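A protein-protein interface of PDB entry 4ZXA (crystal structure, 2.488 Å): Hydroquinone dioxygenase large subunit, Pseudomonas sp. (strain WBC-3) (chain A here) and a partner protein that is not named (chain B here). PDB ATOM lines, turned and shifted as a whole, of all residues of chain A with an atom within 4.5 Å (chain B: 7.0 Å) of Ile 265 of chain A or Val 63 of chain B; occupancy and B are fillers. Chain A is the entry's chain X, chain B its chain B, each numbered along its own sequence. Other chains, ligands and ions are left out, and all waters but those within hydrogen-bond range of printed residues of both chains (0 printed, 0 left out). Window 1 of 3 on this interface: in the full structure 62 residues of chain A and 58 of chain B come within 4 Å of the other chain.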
ATOM      1  N   PHE A 243       3.650  -8.169  -0.709  1.00  0.00           N
ATOM      2  CA  PHE A 243       3.585  -6.749  -0.360  1.00  0.00           C
ATOM      3  C   PHE A 243       4.803  -6.400   0.496  1.00  0.00           C
ATOM      4  O   PHE A 243       4.979  -6.942   1.582  1.00  0.00           O
ATOM      5  CB  PHE A 243       2.284  -6.418   0.387  1.00  0.00           C
ATOM      6  CG  PHE A 243       1.189  -5.890  -0.492  1.00  0.00           C
ATOM      7  CD1 PHE A 243       1.202  -6.110  -1.860  1.00  0.00           C
ATOM      8  CD2 PHE A 243       0.157  -5.145   0.046  1.00  0.00           C
ATOM      9  CE1 PHE A 243       0.191  -5.602  -2.674  1.00  0.00           C
ATOM     10  CE2 PHE A 243      -0.857  -4.639  -0.756  1.00  0.00           C
ATOM     11  CZ  PHE A 243      -0.840  -4.866  -2.117  1.00  0.00           C
ATOM     12  N   TRP A 263       5.686  -2.753  -9.067  1.00  0.00           N
ATOM     13  CA  TRP A 263       4.761  -1.640  -8.894  1.00  0.00           C
ATOM     14  C   TRP A 263       5.017  -0.961  -7.572  1.00  0.00           C
ATOM     15  O   TRP A 263       5.269  -1.616  -6.580  1.00  0.00           O
ATOM     16  CB  TRP A 263       3.329  -2.139  -8.884  1.00  0.00           C
ATOM     17  CG  TRP A 263       2.856  -2.730 -10.169  1.00  0.00           C
ATOM     18  CD1 TRP A 263       3.169  -3.961 -10.676  1.00  0.00           C
ATOM     19  CD2 TRP A 263       1.944  -2.132 -11.099  1.00  0.00           C
ATOM     20  NE1 TRP A 263       2.514  -4.159 -11.873  1.00  0.00           N
ATOM     21  CE2 TRP A 263       1.752  -3.053 -12.150  1.00  0.00           C
ATOM     22  CE3 TRP A 263       1.267  -0.907 -11.140  1.00  0.00           C
ATOM     23  CZ2 TRP A 263       0.918  -2.784 -13.242  1.00  0.00           C
ATOM     24  CZ3 TRP A 263       0.433  -0.640 -12.230  1.00  0.00           C
ATOM     25  CH2 TRP A 263       0.269  -1.578 -13.263  1.00  0.00           C
ATOM     26  N   PHE A 264       4.956   0.360  -7.570  1.00  0.00           N
ATOM     27  CA  PHE A 264       5.060   1.133  -6.355  1.00  0.00           C
ATOM     28  C   PHE A 264       3.698   1.710  -6.059  1.00  0.00           C
ATOM     29  O   PHE A 264       3.026   2.213  -6.968  1.00  0.00           O
ATOM     30  CB  PHE A 264       6.019   2.304  -6.544  1.00  0.00           C
ATOM     31  CG  PHE A 264       7.428   1.901  -6.856  1.00  0.00           C
ATOM     32  CD1 PHE A 264       7.908   0.648  -6.497  1.00  0.00           C
ATOM     33  CD2 PHE A 264       8.282   2.785  -7.504  1.00  0.00           C
ATOM     34  CE1 PHE A 264       9.199   0.285  -6.787  1.00  0.00           C
ATOM     35  CE2 PHE A 264       9.578   2.425  -7.788  1.00  0.00           C
ATOM     36  CZ  PHE A 264      10.035   1.177  -7.430  1.00  0.00           C
ATOM     37  N   ILE A 265       3.286   1.650  -4.795  1.00  0.00           N
ATOM     38  CA  ILE A 265       2.149   2.445  -4.355  1.00  0.00           C
ATOM     39  C   ILE A 265       2.591   3.384  -3.241  1.00  0.00           C
ATOM     40  O   ILE A 265       2.968   2.937  -2.151  1.00  0.00           O
ATOM     41  CB  ILE A 265       0.948   1.581  -3.914  1.00  0.00           C
ATOM     42  CG1 ILE A 265       0.705   0.461  -4.919  1.00  0.00           C
ATOM     43  CG2 ILE A 265      -0.324   2.441  -3.783  1.00  0.00           C
ATOM     44  CD1 ILE A 265      -0.475  -0.425  -4.565  1.00  0.00           C
ATOM     45  N   GLN A 266       2.567   4.688  -3.523  1.00  0.00           N
ATOM     46  CA  GLN A 266       2.994   5.687  -2.538  1.00  0.00           C
ATOM     47  C   GLN A 266       1.892   5.804  -1.481  1.00  0.00           C
ATOM     48  O   GLN A 266       0.726   6.017  -1.828  1.00  0.00           O
ATOM     49  CB  GLN A 266       3.259   7.034  -3.228  1.00  0.00           C
ATOM     50  CG  GLN A 266       4.027   8.059  -2.410  1.00  0.00           C
ATOM     51  CD  GLN A 266       5.406   7.566  -1.983  1.00  0.00           C
ATOM     52  OE1 GLN A 266       6.033   6.773  -2.678  1.00  0.00           O
ATOM     53  NE2 GLN A 266       5.875   8.029  -0.823  1.00  0.00           N
ATOM     54  N   MET A 267       2.240   5.619  -0.207  1.00  0.00           N
ATOM     55  CA  MET A 267       1.230   5.629   0.864  1.00  0.00           C
ATOM     56  C   MET A 267       1.293   6.897   1.712  1.00  0.00           C
ATOM     57  O   MET A 267       0.299   7.292   2.307  1.00  0.00           O
ATOM     58  CB  MET A 267       1.330   4.386   1.760  1.00  0.00           C
ATOM     59  CG  MET A 267       1.103   3.100   1.014  1.00  0.00           C
ATOM     60  SD  MET A 267       0.981   1.644   2.072  1.00  0.00           S
ATOM     61  CE  MET A 267       2.636   1.458   2.683  1.00  0.00           C
ATOM     62  N   ASP A 293      -0.529   7.413  -5.136  1.00  0.00           N
ATOM     63  CA  ASP A 293      -0.149   7.146  -6.523  1.00  0.00           C
ATOM     64  C   ASP A 293       0.259   5.684  -6.745  1.00  0.00           C
ATOM     65  O   ASP A 293       0.737   5.022  -5.827  1.00  0.00           O
ATOM     66  CB  ASP A 293       0.947   8.111  -6.996  1.00  0.00           C
ATOM     67  CG  ASP A 293       0.386   9.463  -7.477  1.00  0.00           C
ATOM     68  OD1 ASP A 293      -0.834   9.533  -7.786  1.00  0.00           O
ATOM     69  OD2 ASP A 293       1.173  10.450  -7.560  1.00  0.00           O
ATOM     70  N   VAL A 294       0.043   5.190  -7.964  1.00  0.00           N
ATOM     71  CA  VAL A 294       0.317   3.801  -8.329  1.00  0.00           C
ATOM     72  C   VAL A 294       1.083   3.777  -9.633  1.00  0.00           C
ATOM     73  O   VAL A 294       0.617   4.283 -10.655  1.00  0.00           O
ATOM     74  CB  VAL A 294      -0.968   3.012  -8.582  1.00  0.00           C
ATOM     75  CG1 VAL A 294      -0.639   1.628  -9.123  1.00  0.00           C
ATOM     76  CG2 VAL A 294      -1.823   2.929  -7.312  1.00  0.00           C
ATOM     77  N   LEU A 313       6.313   3.783   1.600  1.00  0.00           N
ATOM     78  CA  LEU A 313       6.166   3.258   0.249  1.00  0.00           C
ATOM     79  C   LEU A 313       5.809   1.786   0.236  1.00  0.00           C
ATOM     80  O   LEU A 313       6.418   0.982   0.943  1.00  0.00           O
ATOM     81  CB  LEU A 313       7.444   3.474  -0.549  1.00  0.00           C
ATOM     82  CG  LEU A 313       7.485   2.778  -1.906  1.00  0.00           C
ATOM     83  CD1 LEU A 313       6.443   3.355  -2.825  1.00  0.00           C
ATOM     84  CD2 LEU A 313       8.883   2.883  -2.525  1.00  0.00           C
ATOM     85  N   MET A 314       4.814   1.438  -0.573  1.00  0.00           N
ATOM     86  CA  MET A 314       4.483   0.041  -0.803  1.00  0.00           C
ATOM     87  C   MET A 314       5.170  -0.435  -2.076  1.00  0.00           C
ATOM     88  O   MET A 314       4.930   0.101  -3.164  1.00  0.00           O
ATOM     89  CB  MET A 314       2.968  -0.149  -0.940  1.00  0.00           C
ATOM     90  CG  MET A 314       2.568  -1.545  -1.359  1.00  0.00           C
ATOM     91  SD  MET A 314       3.082  -2.802  -0.163  1.00  0.00           S
ATOM     92  CE  MET A 314       2.053  -2.396   1.250  1.00  0.00           C
ATOM     93  N   TRP A 316       5.445  -3.576  -4.499  1.00  0.00           N
ATOM     94  CA  TRP A 316       4.708  -4.794  -4.784  1.00  0.00           C
ATOM     95  C   TRP A 316       5.509  -5.708  -5.708  1.00  0.00           C
ATOM     96  O   TRP A 316       5.730  -5.378  -6.869  1.00  0.00           O
ATOM     97  CB  TRP A 316       3.350  -4.443  -5.399  1.00  0.00           C
ATOM     98  CG  TRP A 316       2.523  -5.638  -5.764  1.00  0.00           C
ATOM     99  CD1 TRP A 316       2.471  -6.814  -5.104  1.00  0.00           C
ATOM    100  CD2 TRP A 316       1.653  -5.772  -6.902  1.00  0.00           C
ATOM    101  NE1 TRP A 316       1.618  -7.683  -5.746  1.00  0.00           N
ATOM    102  CE2 TRP A 316       1.103  -7.065  -6.853  1.00  0.00           C
ATOM    103  CE3 TRP A 316       1.279  -4.920  -7.946  1.00  0.00           C
ATOM    104  CZ2 TRP A 316       0.196  -7.534  -7.810  1.00  0.00           C
ATOM    105  CZ3 TRP A 316       0.382  -5.385  -8.896  1.00  0.00           C
ATOM    106  CH2 TRP A 316      -0.150  -6.680  -8.819  1.00  0.00           C
ATOM    107  N   ILE B  40      -5.127   6.011  -6.379  1.00  0.00           N
ATOM    108  CA  ILE B  40      -6.214   5.215  -5.823  1.00  0.00           C
ATOM    109  C   ILE B  40      -7.406   6.046  -5.352  1.00  0.00           C
ATOM    110  O   ILE B  40      -8.546   5.601  -5.454  1.00  0.00           O
ATOM    111  CB  ILE B  40      -5.745   4.267  -4.701  1.00  0.00           C
ATOM    112  CG1 ILE B  40      -5.337   5.047  -3.442  1.00  0.00           C
ATOM    113  CG2 ILE B  40      -4.631   3.373  -5.206  1.00  0.00           C
ATOM    114  CD1 ILE B  40      -4.843   4.160  -2.271  1.00  0.00           C
ATOM    115  N   LYS B  52     -14.484  -3.735  -7.708  1.00  0.00           N
ATOM    116  CA  LYS B  52     -13.076  -4.105  -7.528  1.00  0.00           C
ATOM    117  C   LYS B  52     -12.192  -3.627  -8.694  1.00  0.00           C
ATOM    118  O   LYS B  52     -11.853  -4.401  -9.602  1.00  0.00           O
ATOM    119  CB  LYS B  52     -12.944  -5.622  -7.306  1.00  0.00           C
ATOM    120  CG  LYS B  52     -13.758  -6.157  -6.123  1.00  0.00           C
ATOM    121  CD  LYS B  52     -13.705  -7.684  -6.031  1.00  0.00           C
ATOM    122  CE  LYS B  52     -12.703  -8.155  -4.966  1.00  0.00           C
ATOM    123  NZ  LYS B  52     -13.154  -7.965  -3.525  1.00  0.00           N
ATOM    124  N   VAL B  53     -11.825  -2.347  -8.669  1.00  0.00           N
ATOM    125  CA  VAL B  53     -11.054  -1.770  -9.769  1.00  0.00           C
ATOM    126  C   VAL B  53      -9.578  -2.140  -9.694  1.00  0.00           C
ATOM    127  O   VAL B  53      -8.903  -1.847  -8.695  1.00  0.00           O
ATOM    128  CB  VAL B  53     -11.183  -0.225  -9.834  1.00  0.00           C
ATOM    129  CG1 VAL B  53     -10.218   0.335 -10.866  1.00  0.00           C
ATOM    130  CG2 VAL B  53     -12.610   0.189 -10.179  1.00  0.00           C
ATOM    131  N   VAL B  54      -9.079  -2.773 -10.755  1.00  0.00           N
ATOM    132  CA  VAL B  54      -7.659  -3.140 -10.841  1.00  0.00           C
ATOM    133  C   VAL B  54      -6.773  -1.924 -11.120  1.00  0.00           C
ATOM    134  O   VAL B  54      -6.923  -1.265 -12.161  1.00  0.00           O
ATOM    135  CB  VAL B  54      -7.398  -4.213 -11.927  1.00  0.00           C
ATOM    136  CG1 VAL B  54      -5.891  -4.438 -12.108  1.00  0.00           C
ATOM    137  CG2 VAL B  54      -8.099  -5.530 -11.568  1.00  0.00           C
ATOM    138  N   VAL B  55      -5.859  -1.630 -10.192  1.00  0.00           N
ATOM    139  CA  VAL B  55      -4.898  -0.537 -10.374  1.00  0.00           C
ATOM    140  C   VAL B  55      -3.461  -1.063 -10.515  1.00  0.00           C
ATOM    141  O   VAL B  55      -2.524  -0.309 -10.797  1.00  0.00           O
ATOM    142  CB  VAL B  55      -4.971   0.494  -9.219  1.00  0.00           C
ATOM    143  CG1 VAL B  55      -6.330   1.183  -9.208  1.00  0.00           C
ATOM    144  CG2 VAL B  55      -4.703  -0.173  -7.886  1.00  0.00           C
ATOM    145  N   GLY B  56      -3.308  -2.367 -10.305  1.00  0.00           N
ATOM    146  CA  GLY B  56      -2.034  -3.041 -10.461  1.00  0.00           C
ATOM    147  C   GLY B  56      -2.241  -4.474 -10.933  1.00  0.00           C
ATOM    148  O   GLY B  56      -3.065  -5.217 -10.397  1.00  0.00           O
ATOM    149  N   LEU B  57      -1.479  -4.857 -11.945  1.00  0.00           N
ATOM    150  CA  LEU B  57      -1.569  -6.179 -12.540  1.00  0.00           C
ATOM    151  C   LEU B  57      -0.159  -6.712 -12.790  1.00  0.00           C
ATOM    152  O   LEU B  57       0.683  -6.016 -13.361  1.00  0.00           O
ATOM    153  CB  LEU B  57      -2.323  -6.096 -13.861  1.00  0.00           C
ATOM    154  CG  LEU B  57      -2.548  -7.388 -14.643  1.00  0.00           C
ATOM    155  CD1 LEU B  57      -3.540  -8.292 -13.923  1.00  0.00           C
ATOM    156  CD2 LEU B  57      -3.036  -7.084 -16.052  1.00  0.00           C
ATOM    157  N   ASN B  58       0.098  -7.935 -12.345  1.00  0.00           N
ATOM    158  CA  ASN B  58       1.395  -8.565 -12.559  1.00  0.00           C
ATOM    159  C   ASN B  58       1.199 -10.054 -12.854  1.00  0.00           C
ATOM    160  O   ASN B  58       1.184 -10.876 -11.951  1.00  0.00           O
ATOM    161  CB  ASN B  58       2.330  -8.333 -11.355  1.00  0.00           C
ATOM    162  CG  ASN B  58       3.808  -8.608 -11.684  1.00  0.00           C
ATOM    163  OD1 ASN B  58       4.127  -9.494 -12.477  1.00  0.00           O
ATOM    164  ND2 ASN B  58       4.708  -7.835 -11.070  1.00  0.00           N
ATOM    165  N   TYR B  61      -1.601 -11.768 -10.860  1.00  0.00           N
ATOM    166  CA  TYR B  61      -1.796 -11.182  -9.538  1.00  0.00           C
ATOM    167  C   TYR B  61      -2.298  -9.776  -9.728  1.00  0.00           C
ATOM    168  O   TYR B  61      -1.964  -9.123 -10.730  1.00  0.00           O
ATOM    169  CB  TYR B  61      -0.506 -11.166  -8.732  1.00  0.00           C
ATOM    170  CG  TYR B  61      -0.002 -12.542  -8.427  1.00  0.00           C
ATOM    171  CD1 TYR B  61      -0.556 -13.282  -7.404  1.00  0.00           C
ATOM    172  CD2 TYR B  61       1.020 -13.119  -9.184  1.00  0.00           C
ATOM    173  CE1 TYR B  61      -0.100 -14.553  -7.124  1.00  0.00           C
ATOM    174  CE2 TYR B  61       1.482 -14.397  -8.907  1.00  0.00           C
ATOM    175  CZ  TYR B  61       0.919 -15.105  -7.870  1.00  0.00           C
ATOM    176  OH  TYR B  61       1.364 -16.378  -7.573  1.00  0.00           O
ATOM    177  N   VAL B  62      -3.087  -9.299  -8.770  1.00  0.00           N
ATOM    178  CA  VAL B  62      -3.650  -7.967  -8.896  1.00  0.00           C
ATOM    179  C   VAL B  62      -3.684  -7.195  -7.582  1.00  0.00           C
ATOM    180  O   VAL B  62      -3.681  -7.765  -6.482  1.00  0.00           O
ATOM    181  CB  VAL B  62      -5.094  -8.011  -9.469  1.00  0.00           C
ATOM    182  CG1 VAL B  62      -5.094  -8.577 -10.865  1.00  0.00           C
ATOM    183  CG2 VAL B  62      -5.989  -8.841  -8.554  1.00  0.00           C
ATOM    184  N   VAL B  63      -3.724  -5.878  -7.724  1.00  0.00           N
ATOM    185  CA  VAL B  63      -4.055  -5.009  -6.617  1.00  0.00           C
ATOM    186  C   VAL B  63      -5.308  -4.229  -7.005  1.00  0.00           C
ATOM    187  O   VAL B  63      -5.337  -3.518  -8.006  1.00  0.00           O
ATOM    188  CB  VAL B  63      -2.877  -4.091  -6.243  1.00  0.00           C
ATOM    189  CG1 VAL B  63      -3.267  -3.144  -5.144  1.00  0.00           C
ATOM    190  CG2 VAL B  63      -1.708  -4.938  -5.792  1.00  0.00           C
ATOM    191  N   GLU B  64      -6.356  -4.402  -6.213  1.00  0.00           N
ATOM    192  CA  GLU B  64      -7.646  -3.805  -6.507  1.00  0.00           C
ATOM    193  C   GLU B  64      -7.874  -2.626  -5.577  1.00  0.00           C
ATOM    194  O   GLU B  64      -7.477  -2.655  -4.410  1.00  0.00           O
ATOM    195  CB  GLU B  64      -8.757  -4.847  -6.336  1.00  0.00           C
ATOM    196  CG  GLU B  64      -8.674  -6.014  -7.323  1.00  0.00           C
ATOM    197  CD  GLU B  64      -9.625  -7.161  -6.985  1.00  0.00           C
ATOM    198  OE1 GLU B  64     -10.003  -7.296  -5.799  1.00  0.00           O
ATOM    199  OE2 GLU B  64      -9.989  -7.933  -7.905  1.00  0.00           O
ATOM    200  N   THR B  65      -8.476  -1.572  -6.113  1.00  0.00           N
ATOM    201  CA  THR B  65      -8.948  -0.461  -5.302  1.00  0.00           C
ATOM    202  C   THR B  65     -10.466  -0.555  -5.231  1.00  0.00           C
ATOM    203  O   THR B  65     -11.142  -0.681  -6.261  1.00  0.00           O
ATOM    204  CB  THR B  65      -8.541   0.916  -5.895  1.00  0.00           C
ATOM    205  OG1 THR B  65      -7.143   1.137  -5.676  1.00  0.00           O
ATOM    206  CG2 THR B  65      -9.311   2.051  -5.225  1.00  0.00           C
ATOM    207  N   LEU B  66     -11.001  -0.518  -4.017  1.00  0.00           N
ATOM    208  CA  LEU B  66     -12.445  -0.546  -3.817  1.00  0.00           C
ATOM    209  C   LEU B  66     -12.884   0.713  -3.101  1.00  0.00           C
ATOM    210  O   LEU B  66     -12.287   1.094  -2.085  1.00  0.00           O
ATOM    211  CB  LEU B  66     -12.872  -1.753  -2.976  1.00  0.00           C
ATOM    212  CG  LEU B  66     -12.702  -3.155  -3.557  1.00  0.00           C
ATOM    213  CD1 LEU B  66     -11.239  -3.582  -3.522  1.00  0.00           C
ATOM    214  CD2 LEU B  66     -13.565  -4.154  -2.782  1.00  0.00           C
ATOM    215  N   MET B  86      -7.147   2.682   3.227  1.00  0.00           N
ATOM    216  CA  MET B  86      -6.356   3.874   2.958  1.00  0.00           C
ATOM    217  C   MET B  86      -7.135   5.143   3.295  1.00  0.00           C
ATOM    218  O   MET B  86      -6.540   6.174   3.594  1.00  0.00           O
ATOM    219  CB  MET B  86      -5.863   3.881   1.510  1.00  0.00           C
ATOM    220  CG  MET B  86      -4.907   2.744   1.183  1.00  0.00           C
ATOM    221  SD  MET B  86      -3.267   2.987   1.908  1.00  0.00           S
ATOM    222  CE  MET B  86      -2.966   4.699   1.491  1.00  0.00           C
ATOM    223  N   LEU B 149      -7.655  -1.076  -0.371  1.00  0.00           N
ATOM    224  CA  LEU B 149      -6.767  -1.760  -1.310  1.00  0.00           C
ATOM    225  C   LEU B 149      -6.804  -3.232  -0.969  1.00  0.00           C
ATOM    226  O   LEU B 149      -6.625  -3.605   0.195  1.00  0.00           O
ATOM    227  CB  LEU B 149      -5.322  -1.272  -1.198  1.00  0.00           C
ATOM    228  CG  LEU B 149      -4.915   0.073  -1.783  1.00  0.00           C
ATOM    229  CD1 LEU B 149      -3.488   0.390  -1.384  1.00  0.00           C
ATOM    230  CD2 LEU B 149      -5.041   0.099  -3.286  1.00  0.00           C
ATOM    231  N   GLN B 150      -7.043  -4.064  -1.976  1.00  0.00           N
ATOM    232  CA  GLN B 150      -7.124  -5.501  -1.771  1.00  0.00           C
ATOM    233  C   GLN B 150      -6.048  -6.204  -2.591  1.00  0.00           C
ATOM    234  O   GLN B 150      -5.891  -5.945  -3.779  1.00  0.00           O
ATOM    235  CB  GLN B 150      -8.527  -6.020  -2.124  1.00  0.00           C
ATOM    236  CG  GLN B 150      -8.714  -7.530  -1.921  1.00  0.00           C
ATOM    237  CD  GLN B 150     -10.175  -7.952  -1.663  1.00  0.00           C
ATOM    238  OE1 GLN B 150     -11.046  -7.116  -1.401  1.00  0.00           O
ATOM    239  NE2 GLN B 150     -10.435  -9.256  -1.736  1.00  0.00           N
ATOM    240  N   GLN B 151      -5.288  -7.073  -1.939  1.00  0.00           N
ATOM    241  CA  GLN B 151      -4.250  -7.835  -2.618  1.00  0.00           C
ATOM    242  C   GLN B 151      -4.808  -9.213  -2.816  1.00  0.00           C
ATOM    243  O   GLN B 151      -5.087  -9.906  -1.844  1.00  0.00           O
ATOM    244  CB  GLN B 151      -2.981  -7.920  -1.763  1.00  0.00           C
ATOM    245  CG  GLN B 151      -1.853  -8.751  -2.361  1.00  0.00           C
ATOM    246  CD  GLN B 151      -0.787  -9.096  -1.326  1.00  0.00           C
ATOM    247  OE1 GLN B 151      -0.880  -8.700  -0.170  1.00  0.00           O
ATOM    248  NE2 GLN B 151       0.225  -9.842  -1.740  1.00  0.00           N
ATOM    249  N   THR B 152      -4.975  -9.609  -4.071  1.00  0.00           N
ATOM    250  CA  THR B 152      -5.563 -10.905  -4.385  1.00  0.00           C
ATOM    251  C   THR B 152      -5.191 -11.272  -5.819  1.00  0.00           C
ATOM    252  O   THR B 152      -4.236 -10.736  -6.364  1.00  0.00           O
ATOM    253  CB  THR B 152      -7.112 -10.900  -4.150  1.00  0.00           C
ATOM    254  OG1 THR B 152      -7.676 -12.173  -4.496  1.00  0.00           O
ATOM    255  CG2 THR B 152      -7.785  -9.805  -4.960  1.00  0.00           C
ATOM    256  N   ILE B 153      -5.942 -12.180  -6.426  1.00  0.00           N
ATOM    257  CA  ILE B 153      -5.661 -12.634  -7.783  1.00  0.00           C
ATOM    258  C   ILE B 153      -6.802 -12.232  -8.728  1.00  0.00           C
ATOM    259  O   ILE B 153      -7.941 -12.117  -8.304  1.00  0.00           O
ATOM    260  CB  ILE B 153      -5.441 -14.171  -7.793  1.00  0.00           C
ATOM    261  CG1 ILE B 153      -4.251 -14.527  -6.896  1.00  0.00           C
ATOM    262  CG2 ILE B 153      -5.268 -14.702  -9.219  1.00  0.00           C
ATOM    263  CD1 ILE B 153      -3.844 -15.985  -6.929  1.00  0.00           C
ATOM    264  N   TRP B 162      -8.173   0.631 -17.671  1.00  0.00           N
ATOM    265  CA  TRP B 162      -6.889   1.329 -17.698  1.00  0.00           C
ATOM    266  C   TRP B 162      -6.907   2.656 -18.462  1.00  0.00           C
ATOM    267  O   TRP B 162      -6.355   3.663 -17.993  1.00  0.00           O
ATOM    268  CB  TRP B 162      -5.795   0.430 -18.277  1.00  0.00           C
ATOM    269  CG  TRP B 162      -5.635  -0.866 -17.574  1.00  0.00           C
ATOM    270  CD1 TRP B 162      -6.105  -2.080 -17.984  1.00  0.00           C
ATOM    271  CD2 TRP B 162      -4.943  -1.099 -16.343  1.00  0.00           C
ATOM    272  NE1 TRP B 162      -5.760  -3.050 -17.083  1.00  0.00           N
ATOM    273  CE2 TRP B 162      -5.040  -2.479 -16.066  1.00  0.00           C
ATOM    274  CE3 TRP B 162      -4.255  -0.278 -15.446  1.00  0.00           C
ATOM    275  CZ2 TRP B 162      -4.478  -3.061 -14.918  1.00  0.00           C
ATOM    276  CZ3 TRP B 162      -3.687  -0.860 -14.305  1.00  0.00           C
ATOM    277  CH2 TRP B 162      -3.815  -2.233 -14.051  1.00  0.00           C
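NE1 of Trp 263 of chain A is in hydrogen-bond range of O of Leu 57 of chain B (3.0 Å).
The backbone NH (N) of Val 55 of chain B lies within hydrogen-bond range of the backbone carbonyl oxygen (O) of Val 63 of chain B, at 2.9 Å.
The backbone NH (N) of Val 63 of chain B sits at hydrogen-bond distance from the backbone carbonyl oxygen (O) of Gly 56 of chain B, at 2.8 Å.
The backbone NH (N) of Val 62 of chain B lies within hydrogen-bond range of the backbone carbonyl oxygen (O) of Thr 152 of chain B, at 3.0 Å.
N of Trp 316 of chain A sits at hydrogen-bond distance from O of Trp 263 of chain A (2.9 Å).
O of Met 314 of chain A is in hydrogen-bond range of N of Ile 265 of chain A (2.8 Å).
Among the printed residues, pairs that only touch across the chains: Phe 243 of chain A with Val 63 of chain B (3.7 Å), Phe 243 of chain A with Gln 151 of chain B (3.5 Å), Trp 263 of chain A with Val 55 of chain B (3.3 Å), Trp 263 of chain A with Gly 56 of chain B (3.9 Å), Ile 265 of chain A with Val 63 of chain B (3.9 Å), Val 294 of chain A with Ile 40 of chain B (3.5 Å), Val 294 of chain A with Val 55 of chain B (3.2 Å), Trp 316 of chain A with Gly 56 of chain B (3.4 Å), Trp 316 of chain A with Leu 57 of chain B (3.6 Å), Trp 316 of chain A with Asn 58 of chain B (3.8 Å), Trp 316 of chain A with Tyr 61 of chain B (3.6 Å), Trp 316 of chain A with Val 62 of chain B (3.7 Å) and Trp 316 of chain A with Val 63 of chain B (3.6 Å).
Ile 265 of chain A touches just one residue of chain B: Val 63.
Val 63 of chain B touches three residues of chain A.
Of the printed residues of chain A, Gln 151 of chain B touches Phe 243.
Printed residues of chain A within 4 Å of Leu 57 of chain B: Trp 263 and Trp 316.
Printed residues of chain B within 4 Å of Trp 316 of chain A: Gly 56, Leu 57, Asn 58, Tyr 61, Val 62 and Val 63.
Glu 64 of chain B touches none of the printed residues of chain A.
Phe 264 of chain A touches none of the printed residues of chain B.
The nearest printed residue of chain A that does not touch Val 62 of chain B is Phe 243 of chain A (5.8 Å).
Of the 21 printed residues of chain B, 9 touch a printed residue of chain A.
Hydrophobic or aromatic side chains of chain B that line the printed part of chain A: Ile 40, Tyr 61 and Val 63.
Of the 11 printed residues of chain A, 5 touch a printed residue of chain B.
Hydrophobic or aromatic side chains of chain A within 4 Å of the printed part of chain B: Phe 243, Trp 263, Ile 265, Val 294 and Trp 316.
Among the printed residues, 14 pairs touch across the chains.
Among the printed residues, no Asp or Glu carboxylate lies within 4 Å of a Lys or Arg side-chain nitrogen of the other chain.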
